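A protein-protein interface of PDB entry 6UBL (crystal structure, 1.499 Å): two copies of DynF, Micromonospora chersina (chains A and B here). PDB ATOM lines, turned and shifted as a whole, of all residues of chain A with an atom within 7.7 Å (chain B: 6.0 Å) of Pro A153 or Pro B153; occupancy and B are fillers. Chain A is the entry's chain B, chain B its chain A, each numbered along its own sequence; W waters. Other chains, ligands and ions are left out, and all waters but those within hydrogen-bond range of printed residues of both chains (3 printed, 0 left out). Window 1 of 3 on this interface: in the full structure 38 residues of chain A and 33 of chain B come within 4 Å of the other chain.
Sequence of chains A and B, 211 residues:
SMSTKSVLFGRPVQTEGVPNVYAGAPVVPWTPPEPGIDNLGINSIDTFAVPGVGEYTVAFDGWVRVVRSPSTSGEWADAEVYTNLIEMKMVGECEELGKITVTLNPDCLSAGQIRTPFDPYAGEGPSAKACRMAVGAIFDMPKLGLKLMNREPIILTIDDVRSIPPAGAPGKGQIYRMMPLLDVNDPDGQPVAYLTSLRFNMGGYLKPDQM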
ATOM      1  N   VAL A   7      -2.098  17.465  -6.995  1.00  0.00           N
ATOM      2  CA  VAL A   7      -2.807  18.114  -8.096  1.00  0.00           C
ATOM      3  C   VAL A   7      -2.050  17.757  -9.358  1.00  0.00           C
ATOM      4  O   VAL A   7      -0.880  18.113  -9.495  1.00  0.00           O
ATOM      5  CB  VAL A   7      -2.851  19.639  -7.906  1.00  0.00           C
ATOM      6  CG1 VAL A   7      -3.511  20.317  -9.112  1.00  0.00           C
ATOM      7  CG2 VAL A   7      -3.580  20.015  -6.618  1.00  0.00           C
ATOM      8  N   LEU A   8      -2.705  17.052 -10.269  1.00  0.00           N
ATOM      9  CA  LEU A   8      -2.088  16.626 -11.521  1.00  0.00           C
ATOM     10  C   LEU A   8      -2.701  17.428 -12.660  1.00  0.00           C
ATOM     11  O   LEU A   8      -3.903  17.307 -12.921  1.00  0.00           O
ATOM     12  CB  LEU A   8      -2.343  15.130 -11.730  1.00  0.00           C
ATOM     13  CG  LEU A   8      -2.005  14.268 -10.518  1.00  0.00           C
ATOM     14  CD1 LEU A   8      -2.315  12.799 -10.759  1.00  0.00           C
ATOM     15  CD2 LEU A   8      -0.531  14.429 -10.137  1.00  0.00           C
ATOM     16  N   PHE A   9      -1.866  18.193 -13.373  1.00  0.00           N
ATOM     17  CA  PHE A   9      -2.340  18.981 -14.501  1.00  0.00           C
ATOM     18  C   PHE A   9      -2.147  18.286 -15.845  1.00  0.00           C
ATOM     19  O   PHE A   9      -2.386  18.903 -16.885  1.00  0.00           O
ATOM     20  CB  PHE A   9      -1.710  20.375 -14.537  1.00  0.00           C
ATOM     21  CG  PHE A   9      -2.139  21.285 -13.411  1.00  0.00           C
ATOM     22  CD1 PHE A   9      -3.465  21.367 -13.038  1.00  0.00           C
ATOM     23  CD2 PHE A   9      -1.215  22.098 -12.771  1.00  0.00           C
ATOM     24  CE1 PHE A   9      -3.867  22.208 -12.014  1.00  0.00           C
ATOM     25  CE2 PHE A   9      -1.607  22.944 -11.751  1.00  0.00           C
ATOM     26  CZ  PHE A   9      -2.932  22.998 -11.375  1.00  0.00           C
ATOM     27  N   CYS A 108       1.973  20.250  -7.279  1.00  0.00           N
ATOM     28  CA  CYS A 108       1.325  20.200  -8.583  1.00  0.00           C
ATOM     29  C   CYS A 108       2.261  19.550  -9.587  1.00  0.00           C
ATOM     30  O   CYS A 108       3.442  19.912  -9.670  1.00  0.00           O
ATOM     31  CB  CYS A 108       1.012  21.619  -9.080  1.00  0.00           C
ATOM     32  SG  CYS A 108      -0.129  22.592  -8.076  1.00  0.00           S
ATOM     33  N   LEU A 109       1.726  18.638 -10.391  1.00  0.00           N
ATOM     34  CA  LEU A 109       2.464  18.110 -11.532  1.00  0.00           C
ATOM     35  C   LEU A 109       2.192  19.031 -12.711  1.00  0.00           C
ATOM     36  O   LEU A 109       1.055  19.118 -13.184  1.00  0.00           O
ATOM     37  CB  LEU A 109       2.027  16.684 -11.857  1.00  0.00           C
ATOM     38  CG  LEU A 109       2.756  16.090 -13.070  1.00  0.00           C
ATOM     39  CD1 LEU A 109       4.212  15.827 -12.730  1.00  0.00           C
ATOM     40  CD2 LEU A 109       2.053  14.821 -13.521  1.00  0.00           C
ATOM     41  N   SER A 110       3.227  19.729 -13.165  1.00  0.00           N
ATOM     42  CA  SER A 110       3.158  20.549 -14.366  1.00  0.00           C
ATOM     43  C   SER A 110       3.509  19.677 -15.566  1.00  0.00           C
ATOM     44  O   SER A 110       4.592  19.078 -15.606  1.00  0.00           O
ATOM     45  CB  SER A 110       4.119  21.732 -14.258  1.00  0.00           C
ATOM     46  OG  SER A 110       3.717  22.630 -13.244  1.00  0.00           O
ATOM     47  N   ALA A 111       2.597  19.594 -16.535  1.00  0.00           N
ATOM     48  CA  ALA A 111       2.704  18.583 -17.571  1.00  0.00           C
ATOM     49  C   ALA A 111       2.184  19.145 -18.890  1.00  0.00           C
ATOM     50  O   ALA A 111       1.312  20.024 -18.923  1.00  0.00           O
ATOM     51  CB  ALA A 111       1.917  17.324 -17.195  1.00  0.00           C
ATOM     52  N   MET A 133       1.962  23.402 -22.131  1.00  0.00           N
ATOM     53  CA  MET A 133       2.349  23.012 -20.784  1.00  0.00           C
ATOM     54  C   MET A 133       1.371  23.656 -19.815  1.00  0.00           C
ATOM     55  O   MET A 133       1.038  24.836 -19.971  1.00  0.00           O
ATOM     56  CB  MET A 133       3.767  23.471 -20.478  1.00  0.00           C
ATOM     57  CG  MET A 133       4.339  23.047 -19.127  1.00  0.00           C
ATOM     58  SD  MET A 133       4.745  21.281 -19.061  1.00  0.00           S
ATOM     59  CE  MET A 133       6.272  21.281 -20.006  1.00  0.00           C
ATOM     60  N   ALA A 134       0.914  22.881 -18.824  1.00  0.00           N
ATOM     61  CA  ALA A 134      -0.007  23.369 -17.804  1.00  0.00           C
ATOM     62  C   ALA A 134       0.762  23.411 -16.489  1.00  0.00           C
ATOM     63  O   ALA A 134       1.227  22.367 -16.009  1.00  0.00           O
ATOM     64  CB  ALA A 134      -1.214  22.442 -17.708  1.00  0.00           C
ATOM     65  N   VAL A 135       0.901  24.605 -15.907  1.00  0.00           N
ATOM     66  CA  VAL A 135       1.901  24.841 -14.870  1.00  0.00           C
ATOM     67  C   VAL A 135       1.270  25.281 -13.552  1.00  0.00           C
ATOM     68  O   VAL A 135       0.431  26.190 -13.516  1.00  0.00           O
ATOM     69  CB  VAL A 135       2.940  25.885 -15.316  1.00  0.00           C
ATOM     70  CG1 VAL A 135       3.927  26.178 -14.190  1.00  0.00           C
ATOM     71  CG2 VAL A 135       3.665  25.407 -16.559  1.00  0.00           C
ATOM     72  N   GLY A 136       1.719  24.656 -12.465  1.00  0.00           N
ATOM     73  CA  GLY A 136       1.452  25.133 -11.119  1.00  0.00           C
ATOM     74  C   GLY A 136       2.688  25.779 -10.516  1.00  0.00           C
ATOM     75  O   GLY A 136       3.687  25.096 -10.253  1.00  0.00           O
ATOM     76  N   ALA A 137       2.632  27.090 -10.281  1.00  0.00           N
ATOM     77  CA  ALA A 137       3.807  27.844  -9.880  1.00  0.00           C
ATOM     78  C   ALA A 137       3.648  28.474  -8.506  1.00  0.00           C
ATOM     79  O   ALA A 137       2.553  28.569  -7.949  1.00  0.00           O
ATOM     80  CB  ALA A 137       4.131  28.937 -10.904  1.00  0.00           C
ATOM     81  N   ASN A 150      -1.064  29.537  -7.866  1.00  0.00           N
ATOM     82  CA  ASN A 150      -2.246  29.431  -8.715  1.00  0.00           C
ATOM     83  C   ASN A 150      -2.886  28.055  -8.567  1.00  0.00           C
ATOM     84  O   ASN A 150      -2.185  27.040  -8.468  1.00  0.00           O
ATOM     85  CB  ASN A 150      -1.884  29.698 -10.186  1.00  0.00           C
ATOM     86  CG  ASN A 150      -0.805  28.766 -10.726  1.00  0.00           C
ATOM     87  OD1 ASN A 150       0.298  28.688 -10.184  1.00  0.00           O
ATOM     88  ND2 ASN A 150      -1.115  28.064 -11.819  1.00  0.00           N
ATOM     89  N   ARG A 151      -4.224  28.042  -8.496  1.00  0.00           N
ATOM     90  CA  ARG A 151      -5.014  26.813  -8.580  1.00  0.00           C
ATOM     91  C   ARG A 151      -5.447  26.473 -10.000  1.00  0.00           C
ATOM     92  O   ARG A 151      -5.489  25.289 -10.361  1.00  0.00           O
ATOM     93  CB  ARG A 151      -6.253  26.901  -7.687  1.00  0.00           C
ATOM     94  CG  ARG A 151      -5.947  26.592  -6.251  1.00  0.00           C
ATOM     95  CD  ARG A 151      -7.152  26.608  -5.336  1.00  0.00           C
ATOM     96  NE  ARG A 151      -6.703  26.192  -4.016  1.00  0.00           N
ATOM     97  CZ  ARG A 151      -7.381  26.339  -2.887  1.00  0.00           C
ATOM     98  NH1 ARG A 151      -8.591  26.886  -2.891  1.00  0.00           N
ATOM     99  NH2 ARG A 151      -6.850  25.930  -1.747  1.00  0.00           N
ATOM    100  N   GLU A 152      -5.785  27.476 -10.808  1.00  0.00           N
ATOM    101  CA  GLU A 152      -5.981  27.225 -12.229  1.00  0.00           C
ATOM    102  C   GLU A 152      -4.594  27.105 -12.849  1.00  0.00           C
ATOM    103  O   GLU A 152      -3.729  27.937 -12.558  1.00  0.00           O
ATOM    104  CB  GLU A 152      -6.642  28.434 -12.907  1.00  0.00           C
ATOM    105  CG  GLU A 152      -8.065  28.759 -12.518  1.00  0.00           C
ATOM    106  CD  GLU A 152      -8.585  30.009 -13.187  1.00  0.00           C
ATOM    107  OE1 GLU A 152      -7.953  30.522 -14.180  1.00  0.00           O
ATOM    108  OE2 GLU A 152      -9.634  30.542 -12.753  1.00  0.00           O
ATOM    109  N   PRO A 153      -4.303  26.063 -13.623  1.00  0.00           N
ATOM    110  CA  PRO A 153      -2.958  25.978 -14.207  1.00  0.00           C
ATOM    111  C   PRO A 153      -2.725  27.119 -15.187  1.00  0.00           C
ATOM    112  O   PRO A 153      -3.634  27.551 -15.905  1.00  0.00           O
ATOM    113  CB  PRO A 153      -2.957  24.622 -14.928  1.00  0.00           C
ATOM    114  CG  PRO A 153      -4.391  24.360 -15.246  1.00  0.00           C
ATOM    115  CD  PRO A 153      -5.192  24.994 -14.126  1.00  0.00           C
ATOM    116  N   ILE A 154      -1.490  27.610 -15.216  1.00  0.00           N
ATOM    117  CA  ILE A 154      -1.080  28.563 -16.241  1.00  0.00           C
ATOM    118  C   ILE A 154      -0.795  27.761 -17.502  1.00  0.00           C
ATOM    119  O   ILE A 154       0.066  26.878 -17.501  1.00  0.00           O
ATOM    120  CB  ILE A 154       0.156  29.355 -15.802  1.00  0.00           C
ATOM    121  CG1 ILE A 154      -0.155  30.137 -14.528  1.00  0.00           C
ATOM    122  CG2 ILE A 154       0.608  30.310 -16.904  1.00  0.00           C
ATOM    123  CD1 ILE A 154       1.061  30.562 -13.760  1.00  0.00           C
ATOM    124  N   ILE A 155      -1.540  28.041 -18.564  1.00  0.00           N
ATOM    125  CA  ILE A 155      -1.423  27.310 -19.823  1.00  0.00           C
ATOM    126  C   ILE A 155      -0.435  28.060 -20.711  1.00  0.00           C
ATOM    127  O   ILE A 155      -0.691  29.204 -21.118  1.00  0.00           O
ATOM    128  CB  ILE A 155      -2.786  27.188 -20.522  1.00  0.00           C
ATOM    129  CG1 ILE A 155      -3.785  26.434 -19.632  1.00  0.00           C
ATOM    130  CG2 ILE A 155      -2.638  26.490 -21.870  1.00  0.00           C
ATOM    131  CD1 ILE A 155      -3.309  25.068 -19.173  1.00  0.00           C
ATOM    132  N   LEU A 156       0.696  27.421 -21.017  1.00  0.00           N
ATOM    133  CA  LEU A 156       1.781  28.038 -21.770  1.00  0.00           C
ATOM    134  C   LEU A 156       1.930  27.295 -23.085  1.00  0.00           C
ATOM    135  O   LEU A 156       2.024  26.061 -23.096  1.00  0.00           O
ATOM    136  CB  LEU A 156       3.068  27.946 -20.970  1.00  0.00           C
ATOM    137  CG  LEU A 156       2.854  28.689 -19.647  1.00  0.00           C
ATOM    138  CD1 LEU A 156       3.743  28.111 -18.563  1.00  0.00           C
ATOM    139  CD2 LEU A 156       3.090  30.176 -19.800  1.00  0.00           C
ATOM    140  N   GLN A 174      -1.887  31.481 -22.002  1.00  0.00           N
ATOM    141  CA  GLN A 174      -3.284  31.593 -22.436  1.00  0.00           C
ATOM    142  C   GLN A 174      -4.131  31.890 -21.200  1.00  0.00           C
ATOM    143  O   GLN A 174      -4.801  31.022 -20.629  1.00  0.00           O
ATOM    144  CB  GLN A 174      -3.728  30.310 -23.132  1.00  0.00           C
ATOM    145  CG  GLN A 174      -2.888  29.947 -24.361  1.00  0.00           C
ATOM    146  CD  GLN A 174      -2.986  30.966 -25.484  1.00  0.00           C
ATOM    147  OE1 GLN A 174      -3.927  31.768 -25.544  1.00  0.00           O
ATOM    148  NE2 GLN A 174      -2.013  30.944 -26.383  1.00  0.00           N
ATOM    149  N   ILE A 175      -4.139  33.169 -20.827  1.00  0.00           N
ATOM    150  CA  ILE A 175      -4.825  33.653 -19.636  1.00  0.00           C
ATOM    151  C   ILE A 175      -5.932  34.574 -20.106  1.00  0.00           C
ATOM    152  O   ILE A 175      -5.669  35.602 -20.737  1.00  0.00           O
ATOM    153  CB  ILE A 175      -3.872  34.404 -18.701  1.00  0.00           C
ATOM    154  CG1 ILE A 175      -2.797  33.445 -18.176  1.00  0.00           C
ATOM    155  CG2 ILE A 175      -4.672  35.048 -17.567  1.00  0.00           C
ATOM    156  CD1 ILE A 175      -1.566  34.154 -17.676  1.00  0.00           C
ATOM    157  N   MET A 179      -5.997  35.536 -13.958  1.00  0.00           N
ATOM    158  CA  MET A 179      -5.638  34.248 -13.357  1.00  0.00           C
ATOM    159  C   MET A 179      -5.424  34.470 -11.861  1.00  0.00           C
ATOM    160  O   MET A 179      -4.448  35.149 -11.476  1.00  0.00           O
ATOM    161  CB  MET A 179      -4.345  33.763 -14.016  1.00  0.00           C
ATOM    162  CG  MET A 179      -3.443  32.888 -13.166  1.00  0.00           C
ATOM    163  SD  MET A 179      -4.127  31.246 -12.905  1.00  0.00           S
ATOM    164  CE  MET A 179      -4.167  30.626 -14.587  1.00  0.00           C
ATOM    165  N   PHE B   9     -10.186  23.820  -7.901  1.00  0.00           N
ATOM    166  CA  PHE B   9      -9.911  24.720  -9.016  1.00  0.00           C
ATOM    167  C   PHE B   9     -10.236  26.179  -8.696  1.00  0.00           C
ATOM    168  O   PHE B   9     -10.208  27.022  -9.600  1.00  0.00           O
ATOM    169  CB  PHE B   9     -10.647  24.288 -10.292  1.00  0.00           C
ATOM    170  CG  PHE B   9     -10.183  22.963 -10.849  1.00  0.00           C
ATOM    171  CD1 PHE B   9      -8.824  22.667 -10.927  1.00  0.00           C
ATOM    172  CD2 PHE B   9     -11.092  22.041 -11.314  1.00  0.00           C
ATOM    173  CE1 PHE B   9      -8.398  21.454 -11.433  1.00  0.00           C
ATOM    174  CE2 PHE B   9     -10.668  20.830 -11.826  1.00  0.00           C
ATOM    175  CZ  PHE B   9      -9.323  20.538 -11.890  1.00  0.00           C
ATOM    176  N   ALA B 134     -14.012  27.435 -13.389  1.00  0.00           N
ATOM    177  CA  ALA B 134     -13.022  26.418 -13.730  1.00  0.00           C
ATOM    178  C   ALA B 134     -13.607  25.065 -13.344  1.00  0.00           C
ATOM    179  O   ALA B 134     -13.918  24.845 -12.171  1.00  0.00           O
ATOM    180  CB  ALA B 134     -11.716  26.668 -12.966  1.00  0.00           C
ATOM    181  N   VAL B 135     -13.781  24.177 -14.325  1.00  0.00           N
ATOM    182  CA  VAL B 135     -14.644  23.013 -14.171  1.00  0.00           C
ATOM    183  C   VAL B 135     -13.887  21.712 -14.373  1.00  0.00           C
ATOM    184  O   VAL B 135     -13.166  21.546 -15.363  1.00  0.00           O
ATOM    185  CB  VAL B 135     -15.841  23.085 -15.134  1.00  0.00           C
ATOM    186  CG1 VAL B 135     -16.694  21.827 -15.056  1.00  0.00           C
ATOM    187  CG2 VAL B 135     -16.683  24.313 -14.832  1.00  0.00           C
ATOM    188  N   GLY B 136     -14.111  20.771 -13.460  1.00  0.00           N
ATOM    189  CA  GLY B 136     -13.716  19.376 -13.640  1.00  0.00           C
ATOM    190  C   GLY B 136     -14.932  18.539 -13.982  1.00  0.00           C
ATOM    191  O   GLY B 136     -15.840  18.396 -13.159  1.00  0.00           O
ATOM    192  N   ASN B 150     -11.306  15.449 -17.442  1.00  0.00           N
ATOM    193  CA  ASN B 150     -10.239  16.417 -17.662  1.00  0.00           C
ATOM    194  C   ASN B 150      -9.474  16.643 -16.363  1.00  0.00           C
ATOM    195  O   ASN B 150     -10.071  16.805 -15.296  1.00  0.00           O
ATOM    196  CB  ASN B 150     -10.787  17.734 -18.211  1.00  0.00           C
ATOM    197  CG  ASN B 150     -11.831  18.365 -17.305  1.00  0.00           C
ATOM    198  OD1 ASN B 150     -12.840  17.747 -16.983  1.00  0.00           O
ATOM    199  ND2 ASN B 150     -11.593  19.617 -16.900  1.00  0.00           N
ATOM    200  N   ARG B 151      -8.148  16.649 -16.463  1.00  0.00           N
ATOM    201  CA  ARG B 151      -7.282  17.059 -15.361  1.00  0.00           C
ATOM    202  C   ARG B 151      -7.004  18.552 -15.375  1.00  0.00           C
ATOM    203  O   ARG B 151      -6.861  19.171 -14.310  1.00  0.00           O
ATOM    204  CB  ARG B 151      -5.952  16.303 -15.416  1.00  0.00           C
ATOM    205  CG  ARG B 151      -6.012  14.907 -14.814  1.00  0.00           C
ATOM    206  CD  ARG B 151      -4.661  14.205 -14.773  1.00  0.00           C
ATOM    207  NE  ARG B 151      -4.767  12.954 -14.020  1.00  0.00           N
ATOM    208  CZ  ARG B 151      -3.848  11.995 -13.999  1.00  0.00           C
ATOM    209  NH1 ARG B 151      -2.714  12.135 -14.674  1.00  0.00           N
ATOM    210  NH2 ARG B 151      -4.049  10.903 -13.277  1.00  0.00           N
ATOM    211  N   GLU B 152      -6.894  19.121 -16.552  1.00  0.00           N
ATOM    212  CA  GLU B 152      -6.809  20.556 -16.714  1.00  0.00           C
ATOM    213  C   GLU B 152      -8.218  21.125 -16.654  1.00  0.00           C
ATOM    214  O   GLU B 152      -9.076  20.701 -17.442  1.00  0.00           O
ATOM    215  CB  GLU B 152      -6.219  20.754 -18.101  1.00  0.00           C
ATOM    216  CG  GLU B 152      -5.978  22.131 -18.548  1.00  0.00           C
ATOM    217  CD  GLU B 152      -5.342  22.118 -19.916  1.00  0.00           C
ATOM    218  OE1 GLU B 152      -4.503  21.225 -20.186  1.00  0.00           O
ATOM    219  OE2 GLU B 152      -5.694  22.984 -20.728  1.00  0.00           O
ATOM    220  N   PRO B 153      -8.502  22.074 -15.765  1.00  0.00           N
ATOM    221  CA  PRO B 153      -9.876  22.568 -15.659  1.00  0.00           C
ATOM    222  C   PRO B 153     -10.309  23.266 -16.940  1.00  0.00           C
ATOM    223  O   PRO B 153      -9.527  23.982 -17.581  1.00  0.00           O
ATOM    224  CB  PRO B 153      -9.821  23.542 -14.475  1.00  0.00           C
ATOM    225  CG  PRO B 153      -8.400  23.974 -14.392  1.00  0.00           C
ATOM    226  CD  PRO B 153      -7.583  22.801 -14.871  1.00  0.00           C
ATOM    227  N   ILE B 154     -11.574  23.052 -17.308  1.00  0.00           N
ATOM    228  CA  ILE B 154     -12.185  23.769 -18.419  1.00  0.00           C
ATOM    229  C   ILE B 154     -12.578  25.152 -17.917  1.00  0.00           C
ATOM    230  O   ILE B 154     -13.370  25.275 -16.975  1.00  0.00           O
ATOM    231  CB  ILE B 154     -13.398  23.006 -18.968  1.00  0.00           C
ATOM    232  CG1 ILE B 154     -12.981  21.635 -19.485  1.00  0.00           C
ATOM    233  CG2 ILE B 154     -14.061  23.829 -20.073  1.00  0.00           C
ATOM    234  CD1 ILE B 154     -14.122  20.645 -19.618  1.00  0.00           C
ATOM    235  N   ILE B 155     -12.025  26.185 -18.543  1.00  0.00           N
ATOM    236  CA  ILE B 155     -12.245  27.561 -18.127  1.00  0.00           C
ATOM    237  C   ILE B 155     -13.427  28.101 -18.928  1.00  0.00           C
ATOM    238  O   ILE B 155     -13.364  28.199 -20.162  1.00  0.00           O
ATOM    239  CB  ILE B 155     -10.992  28.411 -18.367  1.00  0.00           C
ATOM    240  CG1 ILE B 155      -9.789  27.859 -17.581  1.00  0.00           C
ATOM    241  CG2 ILE B 155     -11.286  29.877 -18.055  1.00  0.00           C
ATOM    242  CD1 ILE B 155      -9.988  27.660 -16.095  1.00  0.00           C
ATOM    243  N   MET B 179      -7.914  20.678 -25.504  1.00  0.00           N
ATOM    244  CA  MET B 179      -8.020  20.356 -24.074  1.00  0.00           C
ATOM    245  C   MET B 179      -8.042  18.836 -23.966  1.00  0.00           C
ATOM    246  O   MET B 179      -8.985  18.198 -24.488  1.00  0.00           O
ATOM    247  CB  MET B 179      -9.327  20.949 -23.519  1.00  0.00           C
ATOM    248  CG  MET B 179      -9.989  20.159 -22.390  1.00  0.00           C
ATOM    249  SD  MET B 179      -9.144  20.371 -20.808  1.00  0.00           S
ATOM    250  CE  MET B 179      -9.282  22.143 -20.565  1.00  0.00           C
HETATM  251  O   HOH W   1     -10.082  29.711 -10.122  1.00  0.00           O
HETATM  252  O   HOH W   2      -6.601  17.975 -11.914  1.00  0.00           O
HETATM  253  O   HOH W   3      -3.284  18.956 -19.421  1.00  0.00           O
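Glu A152 touches Ile B155, and with the chains exchanged Ile A155 touches Glu B152.
Pro A153 touches its own counterpart, Pro B153.
Of the 4 pairs that touch across the chains among the printed residues, 3 have their exchanged pair printed and touching as well.
Water W3 bridges OE1 of Glu B152 (2.7 Å) and O of Phe A9 (2.7 Å).
Water W2 bridges O of Arg B151 (2.7 Å) and O of Leu A8 (3.0 Å).
Water W1 bridges O of Phe B9 (2.7 Å) and OE2 of Glu A152 (2.8 Å).
Hydrophobic or aromatic side chains of chain A within 4 Å of the printed part of chain B: Leu A8, Pro A153 and Ile A155.
Pro A153 touches one residue of chain B.
Printed residues of chain A within 4 Å of Pro B153: Pro A153.
Printed residues of chain A within 4 Å of Glu B152: Ile A155.
Of the printed residues of chain A, Arg B151 touches Leu A8 (3.4 Å).
Ser A110 touches none of the printed residues of chain B.
The nearest residue of chain B that does not touch Pro A153 is Glu B152 (4.3 Å).
The nearest residue of chain A that does not touch Pro B153 is Glu A152 (4.6 Å).
The side-chain amide nitrogen (ND2) of Asn B150 is in hydrogen-bond range of the backbone carbonyl oxygen (O) of Glu B152, at 2.8 Å.
The backbone carbonyl oxygen of Ile A155 is in hydrogen-bond range of the backbone NH of Gln A174 (2.7 Å).
The side-chain amide nitrogen of Asn A150 lies within hydrogen-bond range of the backbone carbonyl oxygen of Glu A152 (2.7 Å).
CB of Arg B151 touches O of Leu A8 (3.4 Å).
CD of Glu A152 touches CD1 of Ile B155, 3.99 Å away.
CD of Pro B153 touches CD of Pro A153, at 3.3 Å.
OE2 of Glu B152 touches CD1 of Ile A155 (3.5 Å).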
